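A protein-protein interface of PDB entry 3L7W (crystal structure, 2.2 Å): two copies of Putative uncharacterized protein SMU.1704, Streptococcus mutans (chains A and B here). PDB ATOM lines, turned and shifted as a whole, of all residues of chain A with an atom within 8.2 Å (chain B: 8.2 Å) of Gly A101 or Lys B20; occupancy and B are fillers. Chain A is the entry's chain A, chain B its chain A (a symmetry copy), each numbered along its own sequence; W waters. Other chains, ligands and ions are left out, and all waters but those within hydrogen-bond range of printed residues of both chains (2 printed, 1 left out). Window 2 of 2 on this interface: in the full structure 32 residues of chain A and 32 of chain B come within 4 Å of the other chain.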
ATOM      1  N   THR A  94      22.225  30.177  18.308  1.00  0.00           N
ATOM      2  CA  THR A  94      21.483  30.115  17.080  1.00  0.00           C
ATOM      3  C   THR A  94      20.579  28.896  17.098  1.00  0.00           C
ATOM      4  O   THR A  94      19.411  28.995  16.769  1.00  0.00           O
ATOM      5  CB  THR A  94      22.418  30.120  15.898  1.00  0.00           C
ATOM      6  OG1 THR A  94      23.155  31.349  15.925  1.00  0.00           O
ATOM      7  CG2 THR A  94      21.631  30.040  14.597  1.00  0.00           C
ATOM      8  N   ILE A  95      21.122  27.760  17.521  1.00  0.00           N
ATOM      9  CA  ILE A  95      20.332  26.560  17.684  1.00  0.00           C
ATOM     10  C   ILE A  95      19.213  26.790  18.697  1.00  0.00           C
ATOM     11  O   ILE A  95      18.041  26.552  18.412  1.00  0.00           O
ATOM     12  CB  ILE A  95      21.222  25.393  18.079  1.00  0.00           C
ATOM     13  CG1 ILE A  95      22.059  24.992  16.866  1.00  0.00           C
ATOM     14  CG2 ILE A  95      20.387  24.215  18.561  1.00  0.00           C
ATOM     15  CD1 ILE A  95      22.870  23.754  17.088  1.00  0.00           C
ATOM     16  N   ASP A  96      19.572  27.292  19.868  1.00  0.00           N
ATOM     17  CA  ASP A  96      18.585  27.536  20.907  1.00  0.00           C
ATOM     18  C   ASP A  96      17.572  28.572  20.446  1.00  0.00           C
ATOM     19  O   ASP A  96      16.390  28.477  20.756  1.00  0.00           O
ATOM     20  CB  ASP A  96      19.271  27.998  22.188  1.00  0.00           C
ATOM     21  CG  ASP A  96      20.020  26.882  22.875  1.00  0.00           C
ATOM     22  OD1 ASP A  96      19.841  25.705  22.494  1.00  0.00           O
ATOM     23  OD2 ASP A  96      20.781  27.180  23.805  1.00  0.00           O
ATOM     24  N   GLY A  97      18.049  29.562  19.700  1.00  0.00           N
ATOM     25  CA  GLY A  97      17.187  30.592  19.161  1.00  0.00           C
ATOM     26  C   GLY A  97      16.185  29.998  18.186  1.00  0.00           C
ATOM     27  O   GLY A  97      15.002  30.345  18.199  1.00  0.00           O
ATOM     28  N   ILE A  98      16.663  29.105  17.328  1.00  0.00           N
ATOM     29  CA  ILE A  98      15.788  28.454  16.375  1.00  0.00           C
ATOM     30  C   ILE A  98      14.833  27.556  17.149  1.00  0.00           C
ATOM     31  O   ILE A  98      13.622  27.636  16.994  1.00  0.00           O
ATOM     32  CB  ILE A  98      16.582  27.608  15.390  1.00  0.00           C
ATOM     33  CG1 ILE A  98      17.348  28.510  14.421  1.00  0.00           C
ATOM     34  CG2 ILE A  98      15.651  26.693  14.611  1.00  0.00           C
ATOM     35  CD1 ILE A  98      18.062  27.750  13.319  1.00  0.00           C
ATOM     36  N   VAL A  99      15.397  26.727  18.015  1.00  0.00           N
ATOM     37  CA  VAL A  99      14.624  25.807  18.807  1.00  0.00           C
ATOM     38  C   VAL A  99      13.545  26.480  19.637  1.00  0.00           C
ATOM     39  O   VAL A  99      12.428  25.959  19.741  1.00  0.00           O
ATOM     40  CB  VAL A  99      15.515  24.951  19.680  1.00  0.00           C
ATOM     41  CG1 VAL A  99      14.684  24.248  20.764  1.00  0.00           C
ATOM     42  CG2 VAL A  99      16.238  23.939  18.797  1.00  0.00           C
ATOM     43  N   GLU A 100      13.860  27.640  20.206  1.00  0.00           N
ATOM     44  CA  GLU A 100      12.893  28.347  21.042  1.00  0.00           C
ATOM     45  C   GLU A 100      11.946  29.267  20.269  1.00  0.00           C
ATOM     46  O   GLU A 100      11.007  29.808  20.838  1.00  0.00           O
ATOM     47  CB  GLU A 100      13.598  29.099  22.161  1.00  0.00           C
ATOM     48  CG  GLU A 100      14.040  28.174  23.274  1.00  0.00           C
ATOM     49  CD  GLU A 100      15.334  28.615  23.921  1.00  0.00           C
ATOM     50  OE1 GLU A 100      15.655  29.819  23.835  1.00  0.00           O
ATOM     51  OE2 GLU A 100      16.027  27.758  24.516  1.00  0.00           O
ATOM     52  N   GLY A 101      12.190  29.441  18.977  1.00  0.00           N
ATOM     53  CA  GLY A 101      11.240  30.140  18.128  1.00  0.00           C
ATOM     54  C   GLY A 101      11.604  31.554  17.732  1.00  0.00           C
ATOM     55  O   GLY A 101      10.983  32.125  16.834  1.00  0.00           O
ATOM     56  N   ARG A 102      12.602  32.133  18.394  1.00  0.00           N
ATOM     57  CA  ARG A 102      13.003  33.498  18.082  1.00  0.00           C
ATOM     58  C   ARG A 102      13.586  33.572  16.689  1.00  0.00           C
ATOM     59  O   ARG A 102      13.294  34.486  15.925  1.00  0.00           O
ATOM     60  CB  ARG A 102      14.050  33.998  19.072  1.00  0.00           C
ATOM     61  CG  ARG A 102      13.572  34.040  20.501  1.00  0.00           C
ATOM     62  CD  ARG A 102      14.652  34.593  21.403  1.00  0.00           C
ATOM     63  NE  ARG A 102      15.784  33.679  21.508  1.00  0.00           N
ATOM     64  CZ  ARG A 102      15.785  32.582  22.258  1.00  0.00           C
ATOM     65  NH1 ARG A 102      14.710  32.259  22.973  1.00  0.00           N
ATOM     66  NH2 ARG A 102      16.863  31.816  22.300  1.00  0.00           N
ATOM     67  N   ILE A 103      14.424  32.605  16.358  1.00  0.00           N
ATOM     68  CA  ILE A 103      15.166  32.682  15.117  1.00  0.00           C
ATOM     69  C   ILE A 103      14.467  31.945  13.971  1.00  0.00           C
ATOM     70  O   ILE A 103      14.250  30.742  14.036  1.00  0.00           O
ATOM     71  CB  ILE A 103      16.600  32.167  15.312  1.00  0.00           C
ATOM     72  CG1 ILE A 103      17.315  33.036  16.353  1.00  0.00           C
ATOM     73  CG2 ILE A 103      17.315  32.122  13.979  1.00  0.00           C
ATOM     74  CD1 ILE A 103      18.773  32.686  16.585  1.00  0.00           C
ATOM     75  N   ARG A 104      14.136  32.694  12.924  1.00  0.00           N
ATOM     76  CA  ARG A 104      13.456  32.173  11.742  1.00  0.00           C
ATOM     77  C   ARG A 104      13.993  32.939  10.555  1.00  0.00           C
ATOM     78  O   ARG A 104      14.327  34.118  10.680  1.00  0.00           O
ATOM     79  CB  ARG A 104      11.947  32.426  11.837  1.00  0.00           C
ATOM     80  CG  ARG A 104      11.243  31.573  12.863  1.00  0.00           C
ATOM     81  CD  ARG A 104      11.371  30.098  12.514  1.00  0.00           C
ATOM     82  NE  ARG A 104      10.651  29.265  13.476  1.00  0.00           N
ATOM     83  CZ  ARG A 104      11.204  28.711  14.547  1.00  0.00           C
ATOM     84  NH1 ARG A 104      12.494  28.898  14.795  1.00  0.00           N
ATOM     85  NH2 ARG A 104      10.470  27.975  15.371  1.00  0.00           N
ATOM     86  N   HIS A 105      14.065  32.293   9.400  1.00  0.00           N
ATOM     87  CA  HIS A 105      14.510  32.994   8.205  1.00  0.00           C
ATOM     88  C   HIS A 105      13.609  34.211   7.930  1.00  0.00           C
ATOM     89  O   HIS A 105      12.494  34.303   8.457  1.00  0.00           O
ATOM     90  CB  HIS A 105      14.506  32.049   7.014  1.00  0.00           C
ATOM     91  CG  HIS A 105      13.138  31.786   6.476  1.00  0.00           C
ATOM     92  ND1 HIS A 105      12.274  30.883   7.055  1.00  0.00           N
ATOM     93  CD2 HIS A 105      12.478  32.323   5.425  1.00  0.00           C
ATOM     94  CE1 HIS A 105      11.142  30.871   6.378  1.00  0.00           C
ATOM     95  NE2 HIS A 105      11.240  31.736   5.383  1.00  0.00           N
ATOM     96  N   LEU B  13      16.355  20.377  15.168  1.00  0.00           N
ATOM     97  CA  LEU B  13      15.892  21.669  14.664  1.00  0.00           C
ATOM     98  C   LEU B  13      14.537  21.544  13.979  1.00  0.00           C
ATOM     99  O   LEU B  13      13.649  22.348  14.202  1.00  0.00           O
ATOM    100  CB  LEU B  13      16.921  22.279  13.708  1.00  0.00           C
ATOM    101  CG  LEU B  13      18.213  22.713  14.433  1.00  0.00           C
ATOM    102  CD1 LEU B  13      19.282  23.056  13.432  1.00  0.00           C
ATOM    103  CD2 LEU B  13      17.952  23.896  15.338  1.00  0.00           C
ATOM    104  N   ILE B  14      14.391  20.543  13.123  1.00  0.00           N
ATOM    105  CA  ILE B  14      13.143  20.373  12.402  1.00  0.00           C
ATOM    106  C   ILE B  14      11.995  20.208  13.382  1.00  0.00           C
ATOM    107  O   ILE B  14      11.013  20.938  13.329  1.00  0.00           O
ATOM    108  CB  ILE B  14      13.177  19.140  11.502  1.00  0.00           C
ATOM    109  CG1 ILE B  14      14.103  19.390  10.306  1.00  0.00           C
ATOM    110  CG2 ILE B  14      11.777  18.814  11.035  1.00  0.00           C
ATOM    111  CD1 ILE B  14      14.464  18.147   9.553  1.00  0.00           C
ATOM    112  N   LEU B  15      12.125  19.243  14.283  1.00  0.00           N
ATOM    113  CA  LEU B  15      11.074  19.015  15.262  1.00  0.00           C
ATOM    114  C   LEU B  15      10.819  20.273  16.071  1.00  0.00           C
ATOM    115  O   LEU B  15       9.673  20.616  16.349  1.00  0.00           O
ATOM    116  CB  LEU B  15      11.450  17.861  16.178  1.00  0.00           C
ATOM    117  CG  LEU B  15      10.835  16.500  15.851  1.00  0.00           C
ATOM    118  CD1 LEU B  15      10.519  16.353  14.377  1.00  0.00           C
ATOM    119  CD2 LEU B  15      11.710  15.368  16.358  1.00  0.00           C
ATOM    120  N   ALA B  16      11.887  20.979  16.439  1.00  0.00           N
ATOM    121  CA  ALA B  16      11.726  22.165  17.263  1.00  0.00           C
ATOM    122  C   ALA B  16      10.954  23.202  16.481  1.00  0.00           C
ATOM    123  O   ALA B  16      10.050  23.844  17.020  1.00  0.00           O
ATOM    124  CB  ALA B  16      13.072  22.724  17.717  1.00  0.00           C
ATOM    125  N   ILE B  17      11.310  23.356  15.209  1.00  0.00           N
ATOM    126  CA  ILE B  17      10.682  24.362  14.359  1.00  0.00           C
ATOM    127  C   ILE B  17       9.212  24.014  14.168  1.00  0.00           C
ATOM    128  O   ILE B  17       8.331  24.855  14.318  1.00  0.00           O
ATOM    129  CB  ILE B  17      11.362  24.431  12.996  1.00  0.00           C
ATOM    130  CG1 ILE B  17      12.776  25.015  13.141  1.00  0.00           C
ATOM    131  CG2 ILE B  17      10.560  25.282  12.046  1.00  0.00           C
ATOM    132  CD1 ILE B  17      13.592  24.910  11.893  1.00  0.00           C
ATOM    133  N   VAL B  18       8.962  22.749  13.857  1.00  0.00           N
ATOM    134  CA  VAL B  18       7.621  22.297  13.595  1.00  0.00           C
ATOM    135  C   VAL B  18       6.787  22.388  14.859  1.00  0.00           C
ATOM    136  O   VAL B  18       5.575  22.534  14.784  1.00  0.00           O
ATOM    137  CB  VAL B  18       7.626  20.881  13.026  1.00  0.00           C
ATOM    138  CG1 VAL B  18       6.186  20.377  12.817  1.00  0.00           C
ATOM    139  CG2 VAL B  18       8.388  20.884  11.704  1.00  0.00           C
ATOM    140  N   SER B  19       7.433  22.335  16.020  1.00  0.00           N
ATOM    141  CA  SER B  19       6.680  22.413  17.270  1.00  0.00           C
ATOM    142  C   SER B  19       6.060  23.790  17.453  1.00  0.00           C
ATOM    143  O   SER B  19       5.032  23.914  18.106  1.00  0.00           O
ATOM    144  CB  SER B  19       7.547  22.084  18.483  1.00  0.00           C
ATOM    145  OG  SER B  19       8.297  23.216  18.869  1.00  0.00           O
ATOM    146  N   LYS B  20       6.683  24.826  16.893  1.00  0.00           N
ATOM    147  CA  LYS B  20       6.142  26.175  17.042  1.00  0.00           C
ATOM    148  C   LYS B  20       4.821  26.218  16.311  1.00  0.00           C
ATOM    149  O   LYS B  20       3.773  26.503  16.900  1.00  0.00           O
ATOM    150  CB  LYS B  20       7.088  27.231  16.485  1.00  0.00           C
ATOM    151  CG  LYS B  20       6.733  28.656  16.912  1.00  0.00           C
ATOM    152  CD  LYS B  20       7.642  29.685  16.242  1.00  0.00           C
ATOM    153  CE  LYS B  20       7.185  31.115  16.517  1.00  0.00           C
ATOM    154  NZ  LYS B  20       7.657  32.070  15.461  1.00  0.00           N
ATOM    155  N   HIS B  21       4.882  25.924  15.017  1.00  0.00           N
ATOM    156  CA  HIS B  21       3.676  25.717  14.226  1.00  0.00           C
ATOM    157  C   HIS B  21       3.953  24.720  13.104  1.00  0.00           C
ATOM    158  O   HIS B  21       5.101  24.563  12.675  1.00  0.00           O
ATOM    159  CB  HIS B  21       3.158  27.040  13.647  1.00  0.00           C
ATOM    160  CG  HIS B  21       4.172  27.795  12.841  1.00  0.00           C
ATOM    161  ND1 HIS B  21       4.421  27.524  11.513  1.00  0.00           N
ATOM    162  CD2 HIS B  21       4.985  28.828  13.173  1.00  0.00           C
ATOM    163  CE1 HIS B  21       5.348  28.350  11.063  1.00  0.00           C
ATOM    164  NE2 HIS B  21       5.708  29.151  12.049  1.00  0.00           N
ATOM    165  N   ASP B  22       2.905  24.041  12.647  1.00  0.00           N
ATOM    166  CA  ASP B  22       2.997  23.264  11.426  1.00  0.00           C
ATOM    167  C   ASP B  22       3.700  24.115  10.383  1.00  0.00           C
ATOM    168  O   ASP B  22       3.423  25.301  10.262  1.00  0.00           O
ATOM    169  CB  ASP B  22       1.614  22.918  10.913  1.00  0.00           C
ATOM    170  CG  ASP B  22       0.861  22.003  11.842  1.00  0.00           C
ATOM    171  OD1 ASP B  22       1.405  21.650  12.910  1.00  0.00           O
ATOM    172  OD2 ASP B  22      -0.282  21.639  11.496  1.00  0.00           O
ATOM    173  N   SER B  23       4.608  23.518   9.624  1.00  0.00           N
ATOM    174  CA  SER B  23       5.257  24.260   8.545  1.00  0.00           C
ATOM    175  C   SER B  23       5.627  23.400   7.351  1.00  0.00           C
ATOM    176  O   SER B  23       5.847  22.197   7.474  1.00  0.00           O
ATOM    177  CB  SER B  23       6.476  25.040   9.058  1.00  0.00           C
ATOM    178  OG  SER B  23       6.757  24.739  10.412  1.00  0.00           O
ATOM    179  N   THR B  31      14.953  28.205   7.608  1.00  0.00           N
ATOM    180  CA  THR B  31      15.321  28.568   8.961  1.00  0.00           C
ATOM    181  C   THR B  31      16.518  27.745   9.375  1.00  0.00           C
ATOM    182  O   THR B  31      17.385  28.208  10.106  1.00  0.00           O
ATOM    183  CB  THR B  31      14.184  28.335   9.943  1.00  0.00           C
ATOM    184  OG1 THR B  31      13.232  29.390   9.806  1.00  0.00           O
ATOM    185  CG2 THR B  31      14.717  28.329  11.367  1.00  0.00           C
ATOM    186  N   LEU B  73       4.051  18.310  14.232  1.00  0.00           N
ATOM    187  CA  LEU B  73       4.666  17.538  15.292  1.00  0.00           C
ATOM    188  C   LEU B  73       3.624  16.664  15.989  1.00  0.00           C
ATOM    189  O   LEU B  73       2.703  17.168  16.620  1.00  0.00           O
ATOM    190  CB  LEU B  73       5.306  18.487  16.303  1.00  0.00           C
ATOM    191  CG  LEU B  73       6.264  17.837  17.294  1.00  0.00           C
ATOM    192  CD1 LEU B  73       7.377  17.096  16.549  1.00  0.00           C
ATOM    193  CD2 LEU B  73       6.841  18.903  18.239  1.00  0.00           C
ATOM    194  N   GLU B  78       6.451  15.251  19.893  1.00  0.00           N
ATOM    195  CA  GLU B  78       6.604  16.128  21.041  1.00  0.00           C
ATOM    196  C   GLU B  78       7.437  15.449  22.108  1.00  0.00           C
ATOM    197  O   GLU B  78       8.401  16.024  22.601  1.00  0.00           O
ATOM    198  CB  GLU B  78       5.255  16.575  21.604  1.00  0.00           C
ATOM    199  CG  GLU B  78       4.687  17.821  20.934  1.00  0.00           C
ATOM    200  CD  GLU B  78       3.274  18.161  21.402  1.00  0.00           C
ATOM    201  OE1 GLU B  78       2.857  17.673  22.477  1.00  0.00           O
ATOM    202  OE2 GLU B  78       2.578  18.921  20.691  1.00  0.00           O
ATOM    203  N   LEU B  81      10.953  15.329  20.893  1.00  0.00           N
ATOM    204  CA  LEU B  81      11.581  16.638  20.886  1.00  0.00           C
ATOM    205  C   LEU B  81      12.141  16.982  22.272  1.00  0.00           C
ATOM    206  O   LEU B  81      13.200  17.606  22.383  1.00  0.00           O
ATOM    207  CB  LEU B  81      10.599  17.710  20.421  1.00  0.00           C
ATOM    208  CG  LEU B  81      11.075  19.156  20.575  1.00  0.00           C
ATOM    209  CD1 LEU B  81      12.349  19.383  19.763  1.00  0.00           C
ATOM    210  CD2 LEU B  81       9.982  20.131  20.156  1.00  0.00           C
HETATM  211  O   HOH W   1       7.906  27.379  12.851  1.00  0.00           O
HETATM  212  O   HOH W   2       8.065  30.648  11.956  1.00  0.00           O
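The backbone NH (N) of His A105 is in hydrogen-bond range of the side-chain hydroxyl (OG1) of Thr B31.
The backbone carbonyl oxygen of Gly A97 lies within hydrogen-bond range of the backbone NH of Ile A103 (3.0 Å).
The backbone carbonyl oxygen (O) of Ile A98 lies within hydrogen-bond range of the guanidinium group (NH1) of Arg A104 (2.8 Å).
O of Ala B16 lies within hydrogen-bond range of OG of Ser B19 (2.6 Å).
Among the printed residues, pairs that only touch across the chains: Ile A98 with Leu B13, Ile A98 with Ile B17, Ile A98 with Thr B31, Val A99 with Leu B13, Val A99 with Ala B16, Gly A101 with Lys B20, Ile A103 with Thr B31, Arg A104 with Ile B17, Arg A104 with Lys B20 and Arg A104 with Thr B31.
Ile A95 touches none of the printed residues of chain B.
Asp A96 touches none of the printed residues of chain B.
Printed residues of chain B within 4 Å of Ile A98: Leu B13, Ile B17 and Thr B31.
Printed residues of chain B within 4 Å of Val A99: Leu B13 and Ala B16.
Gly A101 touches just one residue of chain B: Lys B20.
Printed residues of chain A within 4 Å of Leu B13: Ile A98 (3.7 Å) and Val A99 (3.9 Å).
Printed residues of chain A within 4 Å of Ile B17: Ile A98 and Arg A104.
No residue of chain A comes within 4 Å of Ser B19.
Lys B20 touches just these residues of chain A: Gly A101 (3.6 Å) and Arg A104 (3.4 Å).
The nearest printed residue of chain B that does not touch Val A99 is Ser B19 (5.0 Å).
Hydrophobic or aromatic side chains of chain A that line the printed part of chain B: Ile A98, Val A99 and His A105.
Of the 15 printed residues of chain B, 5 touch a printed residue of chain A.
Hydrophobic or aromatic side chains of chain B that line the printed part of chain A: Leu B13, Ala B16 and Ile B17.
Among the printed residues, 11 pairs touch across the chains.
Among the printed residues, no Asp or Glu carboxylate lies within 4 Å of a Lys or Arg side-chain nitrogen of the other chain.
No position is printed for both chains.
Of the 11 pairs that touch across the chains among the printed residues, none has its exchanged pair printed and touching as well.
Water W2 bridges a ring nitrogen (NE2) of His B21 (2.8 Å) and the guanidinium group of Arg A104 (3.3 Å).
Water W1 lies within hydrogen-bond range of NE2 of His B21, O of Ile B17 and NE of Arg A104.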
